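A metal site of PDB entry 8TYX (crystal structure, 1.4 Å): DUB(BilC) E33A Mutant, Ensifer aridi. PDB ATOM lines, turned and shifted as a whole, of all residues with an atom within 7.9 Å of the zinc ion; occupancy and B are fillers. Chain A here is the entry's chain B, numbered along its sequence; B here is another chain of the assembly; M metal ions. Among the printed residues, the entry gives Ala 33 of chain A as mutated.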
ATOM      1  N   ALA A  33      24.908  28.110  10.455  1.00  0.00           N
ATOM      2  CA  ALA A  33      24.626  26.706  10.199  1.00  0.00           C
ATOM      3  C   ALA A  33      25.273  26.317   8.871  1.00  0.00           C
ATOM      4  O   ALA A  33      25.368  27.120   7.957  1.00  0.00           O
ATOM      5  CB  ALA A  33      23.126  26.480  10.131  1.00  0.00           C
ATOM      6  N   VAL A  66      19.193  31.290  12.293  1.00  0.00           N
ATOM      7  CA  VAL A  66      19.991  31.254  11.075  1.00  0.00           C
ATOM      8  C   VAL A  66      19.526  30.097  10.207  1.00  0.00           C
ATOM      9  O   VAL A  66      18.896  29.139  10.684  1.00  0.00           O
ATOM     10  CB  VAL A  66      21.499  31.150  11.360  1.00  0.00           C
ATOM     11  CG1 VAL A  66      21.972  32.387  12.103  1.00  0.00           C
ATOM     12  CG2 VAL A  66      21.823  29.893  12.139  1.00  0.00           C
ATOM     13  N   CYS A  67      19.815  30.211   8.926  1.00  0.00           N
ATOM     14  CA  CYS A  67      19.564  29.107   8.020  1.00  0.00           C
ATOM     15  C   CYS A  67      20.665  29.001   6.968  1.00  0.00           C
ATOM     16  O   CYS A  67      21.482  29.905   6.772  1.00  0.00           O
ATOM     17  CB  CYS A  67      18.199  29.171   7.364  1.00  0.00           C
ATOM     18  SG  CYS A  67      18.088  30.305   6.038  1.00  0.00           S
ATOM     19  N   VAL A  68      20.666  27.863   6.293  1.00  0.00           N
ATOM     20  CA  VAL A  68      21.586  27.569   5.207  1.00  0.00           C
ATOM     21  C   VAL A  68      20.744  27.223   3.986  1.00  0.00           C
ATOM     22  O   VAL A  68      19.805  26.440   4.077  1.00  0.00           O
ATOM     23  CB  VAL A  68      22.590  26.459   5.587  1.00  0.00           C
ATOM     24  CG1 VAL A  68      21.935  25.174   6.084  1.00  0.00           C
ATOM     25  CG2 VAL A  68      23.508  26.171   4.401  1.00  0.00           C
ATOM     26  N   GLN A  92      21.288  14.137   4.183  1.00  0.00           N
ATOM     27  CA  GLN A  92      21.747  15.479   4.452  1.00  0.00           C
ATOM     28  C   GLN A  92      22.096  15.608   5.930  1.00  0.00           C
ATOM     29  O   GLN A  92      21.544  14.898   6.778  1.00  0.00           O
ATOM     30  CB  GLN A  92      20.721  16.533   4.052  1.00  0.00           C
ATOM     31  CG  GLN A  92      19.396  16.404   4.750  1.00  0.00           C
ATOM     32  CD  GLN A  92      18.414  17.466   4.271  1.00  0.00           C
ATOM     33  OE1 GLN A  92      18.228  17.640   3.082  1.00  0.00           O
ATOM     34  NE2 GLN A  92      17.791  18.183   5.231  1.00  0.00           N
ATOM     35  N   HIS A  94      23.050  18.841   8.813  1.00  0.00           N
ATOM     36  CA  HIS A  94      23.181  20.269   9.097  1.00  0.00           C
ATOM     37  C   HIS A  94      23.358  20.488  10.581  1.00  0.00           C
ATOM     38  O   HIS A  94      23.107  19.598  11.388  1.00  0.00           O
ATOM     39  CB  HIS A  94      22.080  21.120   8.492  1.00  0.00           C
ATOM     40  CG  HIS A  94      20.793  21.139   9.253  1.00  0.00           C
ATOM     41  ND1 HIS A  94      19.856  20.149   9.169  1.00  0.00           N
ATOM     42  CD2 HIS A  94      20.256  22.067  10.105  1.00  0.00           C
ATOM     43  CE1 HIS A  94      18.800  20.461   9.909  1.00  0.00           C
ATOM     44  NE2 HIS A  94      18.986  21.645  10.476  1.00  0.00           N
ATOM     45  N   SER A  95      23.851  21.662  10.924  1.00  0.00           N
ATOM     46  CA  SER A  95      24.104  22.042  12.300  1.00  0.00           C
ATOM     47  C   SER A  95      23.069  23.027  12.819  1.00  0.00           C
ATOM     48  O   SER A  95      22.453  23.784  12.064  1.00  0.00           O
ATOM     49  CB  SER A  95      25.509  22.636  12.425  1.00  0.00           C
ATOM     50  OG  SER A  95      25.677  23.673  11.518  1.00  0.00           O
ATOM     51  N   HIS A  96      22.907  22.984  14.136  1.00  0.00           N
ATOM     52  CA  HIS A  96      22.120  23.945  14.894  1.00  0.00           C
ATOM     53  C   HIS A  96      23.019  24.725  15.840  1.00  0.00           C
ATOM     54  O   HIS A  96      24.051  24.223  16.284  1.00  0.00           O
ATOM     55  CB  HIS A  96      21.083  23.221  15.736  1.00  0.00           C
ATOM     56  CG  HIS A  96      19.821  22.932  14.981  1.00  0.00           C
ATOM     57  ND1 HIS A  96      18.641  22.574  15.596  1.00  0.00           N
ATOM     58  CD2 HIS A  96      19.557  22.962  13.663  1.00  0.00           C
ATOM     59  CE1 HIS A  96      17.703  22.392  14.700  1.00  0.00           C
ATOM     60  NE2 HIS A  96      18.220  22.629  13.507  1.00  0.00           N
ATOM     61  N   PRO A  97      22.612  25.948  16.201  1.00  0.00           N
ATOM     62  CA  PRO A  97      23.380  26.738  17.176  1.00  0.00           C
ATOM     63  C   PRO A  97      23.378  26.107  18.556  1.00  0.00           C
ATOM     64  O   PRO A  97      24.386  26.197  19.272  1.00  0.00           O
ATOM     65  CB  PRO A  97      22.681  28.109  17.186  1.00  0.00           C
ATOM     66  CG  PRO A  97      21.258  27.786  16.770  1.00  0.00           C
ATOM     67  CD  PRO A  97      21.382  26.644  15.763  1.00  0.00           C
ATOM     68  N   ARG A  99      20.543  23.034  20.708  1.00  0.00           N
ATOM     69  CA  ARG A  99      19.995  21.685  20.684  1.00  0.00           C
ATOM     70  C   ARG A  99      19.640  21.294  19.256  1.00  0.00           C
ATOM     71  O   ARG A  99      19.201  22.120  18.450  1.00  0.00           O
ATOM     72  CB  ARG A  99      18.712  21.638  21.542  1.00  0.00           C
ATOM     73  CG  ARG A  99      17.790  20.386  21.426  1.00  0.00           C
ATOM     74  CD  ARG A  99      16.455  20.494  22.245  1.00  0.00           C
ATOM     75  NE  ARG A  99      15.421  21.304  21.587  1.00  0.00           N
ATOM     76  CZ  ARG A  99      14.414  20.817  20.868  1.00  0.00           C
ATOM     77  NH1 ARG A  99      14.241  19.509  20.698  1.00  0.00           N
ATOM     78  NH2 ARG A  99      13.538  21.665  20.314  1.00  0.00           N
ATOM     79  N   ALA A 100      19.818  20.010  18.935  1.00  0.00           N
ATOM     80  CA  ALA A 100      19.530  19.464  17.608  1.00  0.00           C
ATOM     81  C   ALA A 100      18.124  18.866  17.570  1.00  0.00           C
ATOM     82  O   ALA A 100      17.698  18.179  18.512  1.00  0.00           O
ATOM     83  CB  ALA A 100      20.547  18.373  17.256  1.00  0.00           C
ATOM     84  N   TYR A 101      17.403  19.147  16.482  1.00  0.00           N
ATOM     85  CA  TYR A 101      16.041  18.699  16.238  1.00  0.00           C
ATOM     86  C   TYR A 101      15.743  19.051  14.770  1.00  0.00           C
ATOM     87  O   TYR A 101      16.499  19.786  14.133  1.00  0.00           O
ATOM     88  CB  TYR A 101      15.022  19.339  17.202  1.00  0.00           C
ATOM     89  CG  TYR A 101      15.004  20.840  17.122  1.00  0.00           C
ATOM     90  CD1 TYR A 101      15.919  21.603  17.831  1.00  0.00           C
ATOM     91  CD2 TYR A 101      14.094  21.513  16.334  1.00  0.00           C
ATOM     92  CE1 TYR A 101      15.930  22.993  17.727  1.00  0.00           C
ATOM     93  CE2 TYR A 101      14.097  22.883  16.235  1.00  0.00           C
ATOM     94  CZ  TYR A 101      15.007  23.619  16.925  1.00  0.00           C
ATOM     95  OH  TYR A 101      15.019  24.996  16.834  1.00  0.00           O
ATOM     96  N   HIS A 102      14.607  18.567  14.267  1.00  0.00           N
ATOM     97  CA  HIS A 102      14.121  18.960  12.936  1.00  0.00           C
ATOM     98  C   HIS A 102      13.082  20.069  13.114  1.00  0.00           C
ATOM     99  O   HIS A 102      11.990  19.844  13.665  1.00  0.00           O
ATOM    100  CB  HIS A 102      13.559  17.760  12.156  1.00  0.00           C
ATOM    101  CG  HIS A 102      14.123  17.604  10.772  1.00  0.00           C
ATOM    102  ND1 HIS A 102      13.353  17.603   9.628  1.00  0.00           N
ATOM    103  CD2 HIS A 102      15.406  17.418  10.367  1.00  0.00           C
ATOM    104  CE1 HIS A 102      14.124  17.423   8.578  1.00  0.00           C
ATOM    105  NE2 HIS A 102      15.380  17.318   8.990  1.00  0.00           N
ATOM    106  N   SER A 103      13.410  21.265  12.645  1.00  0.00           N
ATOM    107  CA  SER A 103      12.480  22.383  12.690  1.00  0.00           C
ATOM    108  C   SER A 103      11.427  22.275  11.594  1.00  0.00           C
ATOM    109  O   SER A 103      11.509  21.450  10.677  1.00  0.00           O
ATOM    110  CB  SER A 103      13.252  23.690  12.491  1.00  0.00           C
ATOM    111  OG  SER A 103      13.732  23.769  11.161  1.00  0.00           O
ATOM    112  N   THR A 104      10.415  23.154  11.662  1.00  0.00           N
ATOM    113  CA  THR A 104       9.411  23.187  10.611  1.00  0.00           C
ATOM    114  C   THR A 104      10.041  23.537   9.260  1.00  0.00           C
ATOM    115  O   THR A 104       9.631  23.000   8.229  1.00  0.00           O
ATOM    116  CB  THR A 104       8.289  24.169  10.953  1.00  0.00           C
ATOM    117  OG1 THR A 104       8.829  25.482  11.081  1.00  0.00           O
ATOM    118  CG2 THR A 104       7.646  23.810  12.232  1.00  0.00           C
ATOM    119  N   THR A 105      11.044  24.412   9.248  1.00  0.00           N
ATOM    120  CA  THR A 105      11.763  24.735   8.010  1.00  0.00           C
ATOM    121  C   THR A 105      12.511  23.507   7.501  1.00  0.00           C
ATOM    122  O   THR A 105      12.459  23.189   6.300  1.00  0.00           O
ATOM    123  CB  THR A 105      12.741  25.879   8.258  1.00  0.00           C
ATOM    124  OG1 THR A 105      12.020  27.067   8.611  1.00  0.00           O
ATOM    125  CG2 THR A 105      13.591  26.193   7.042  1.00  0.00           C
ATOM    126  N   ASP A 106      13.186  22.790   8.413  1.00  0.00           N
ATOM    127  CA  ASP A 106      13.892  21.566   8.035  1.00  0.00           C
ATOM    128  C   ASP A 106      12.940  20.572   7.394  1.00  0.00           C
ATOM    129  O   ASP A 106      13.272  19.928   6.375  1.00  0.00           O
ATOM    130  CB  ASP A 106      14.512  20.934   9.296  1.00  0.00           C
ATOM    131  CG  ASP A 106      15.647  21.768   9.910  1.00  0.00           C
ATOM    132  OD1 ASP A 106      16.203  22.625   9.224  1.00  0.00           O
ATOM    133  OD2 ASP A 106      15.954  21.536  11.122  1.00  0.00           O
ATOM    134  N   ASP A 107      11.725  20.448   7.974  1.00  0.00           N
ATOM    135  CA  ASP A 107      10.735  19.498   7.470  1.00  0.00           C
ATOM    136  C   ASP A 107      10.287  19.840   6.053  1.00  0.00           C
ATOM    137  O   ASP A 107       9.907  18.940   5.303  1.00  0.00           O
ATOM    138  CB  ASP A 107       9.458  19.510   8.338  1.00  0.00           C
ATOM    139  CG  ASP A 107       9.623  18.817   9.673  1.00  0.00           C
ATOM    140  OD1 ASP A 107      10.607  18.084   9.867  1.00  0.00           O
ATOM    141  OD2 ASP A 107       8.709  19.006  10.508  1.00  0.00           O
ATOM    142  N   SER A 119      18.165  12.660   7.416  1.00  0.00           N
ATOM    143  CA  SER A 119      18.504  14.052   7.712  1.00  0.00           C
ATOM    144  C   SER A 119      18.997  14.099   9.154  1.00  0.00           C
ATOM    145  O   SER A 119      18.248  13.788  10.073  1.00  0.00           O
ATOM    146  CB  SER A 119      17.281  14.935   7.516  1.00  0.00           C
ATOM    147  OG  SER A 119      17.610  16.275   7.827  1.00  0.00           O
ATOM    148  N   LEU A 120      20.285  14.367   9.306  1.00  0.00           N
ATOM    149  CA  LEU A 120      20.933  14.386  10.610  1.00  0.00           C
ATOM    150  C   LEU A 120      21.196  15.829  11.028  1.00  0.00           C
ATOM    151  O   LEU A 120      21.625  16.640  10.208  1.00  0.00           O
ATOM    152  CB  LEU A 120      22.253  13.616  10.600  1.00  0.00           C
ATOM    153  CG  LEU A 120      22.177  12.106  10.809  1.00  0.00           C
ATOM    154  CD1 LEU A 120      21.363  11.412   9.770  1.00  0.00           C
ATOM    155  CD2 LEU A 120      23.572  11.490  10.864  1.00  0.00           C
ATOM    156  N   VAL A 121      20.998  16.113  12.305  1.00  0.00           N
ATOM    157  CA  VAL A 121      21.169  17.452  12.872  1.00  0.00           C
ATOM    158  C   VAL A 121      22.215  17.364  13.987  1.00  0.00           C
ATOM    159  O   VAL A 121      22.064  16.581  14.949  1.00  0.00           O
ATOM    160  CB  VAL A 121      19.844  18.057  13.362  1.00  0.00           C
ATOM    161  CG1 VAL A 121      20.040  19.524  13.671  1.00  0.00           C
ATOM    162  CG2 VAL A 121      18.744  17.865  12.323  1.00  0.00           C
ATOM    163  N   VAL A 122      23.252  18.170  13.871  1.00  0.00           N
ATOM    164  CA  VAL A 122      24.401  18.172  14.782  1.00  0.00           C
ATOM    165  C   VAL A 122      24.246  19.371  15.709  1.00  0.00           C
ATOM    166  O   VAL A 122      24.132  20.509  15.211  1.00  0.00           O
ATOM    167  CB  VAL A 122      25.720  18.234  14.001  1.00  0.00           C
ATOM    168  CG1 VAL A 122      26.898  18.281  14.937  1.00  0.00           C
ATOM    169  CG2 VAL A 122      25.838  17.052  13.061  1.00  0.00           C
ATOM    170  N   VAL B  95      16.709  24.263   1.938  1.00  0.00           N
ATOM    171  CA  VAL B  95      16.924  25.106   3.109  1.00  0.00           C
ATOM    172  C   VAL B  95      16.926  24.212   4.349  1.00  0.00           C
ATOM    173  O   VAL B  95      16.077  23.323   4.472  1.00  0.00           O
ATOM    174  CB  VAL B  95      15.821  26.186   3.262  1.00  0.00           C
ATOM    175  CG1 VAL B  95      16.148  27.178   4.377  1.00  0.00           C
ATOM    176  CG2 VAL B  95      15.625  26.938   1.971  1.00  0.00           C
ATOM    177  N   ALA B  96      17.833  24.513   5.291  1.00  0.00           N
ATOM    178  CA  ALA B  96      17.799  23.946   6.614  1.00  0.00           C
ATOM    179  C   ALA B  96      18.117  25.035   7.630  1.00  0.00           C
ATOM    180  O   ALA B  96      18.779  26.037   7.316  1.00  0.00           O
ATOM    181  CB  ALA B  96      18.812  22.816   6.851  1.00  0.00           C
ATOM    182  N   GLY B  97      17.743  24.786   8.864  1.00  0.00           N
ATOM    183  CA  GLY B  97      17.929  25.752   9.924  1.00  0.00           C
ATOM    184  C   GLY B  97      16.742  25.493  10.825  1.00  0.00           C
ATOM    185  O   GLY B  97      15.680  26.129  10.728  1.00  0.00           O
HETATM  186 ZN    ZN M   1      17.522  22.633  11.562  1.00  0.00          ZN
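The zinc ion is bound by OD2 of Asp 106 (2.0 Å), NE2 of His 96 of chain A (2.1 Å) and NE2 of His 94 (2.1 Å). Slightly farther from the zinc ion lies the side-chain carboxylate (OD1) of Asp 106 (2.7 Å).
The side-chain carboxylate (OD1) of Asp 106 is in hydrogen-bond range of the backbone NH (N) of Gly 97 of chain B (2.7 Å). O of Tyr 101 lies close to NE2 of His 96 of chain A, 3.4 Å away. O of Arg 99 lies within hydrogen-bond range of ND1 of His 96 of chain A, 2.9 Å away. The backbone NH (N) of His 96 of chain A sits at hydrogen-bond distance from the backbone carbonyl oxygen (O) of Val 122 (3.0 Å). The backbone carbonyl oxygen (O) of Leu 120 lies within hydrogen-bond range of the backbone NH (N) of His 94. O of His 94 is in hydrogen-bond range of N of Val 122. The backbone carbonyl oxygen of Gly 97 of chain B sits at hydrogen-bond distance from the side-chain hydroxyl of Ser 103, 3.1 Å away. OG of Ser 103 sits close to N of Thr 105 (3.4 Å).
Merely in contact with the zinc ion: Gly 97 of chain B, Tyr 101 and Ser 103. Of the 25 residues printed, 6 come within 4 Å of the zinc ion. The nearest printed residue that does not touch the zinc ion is Val 121 (4.5 Å).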
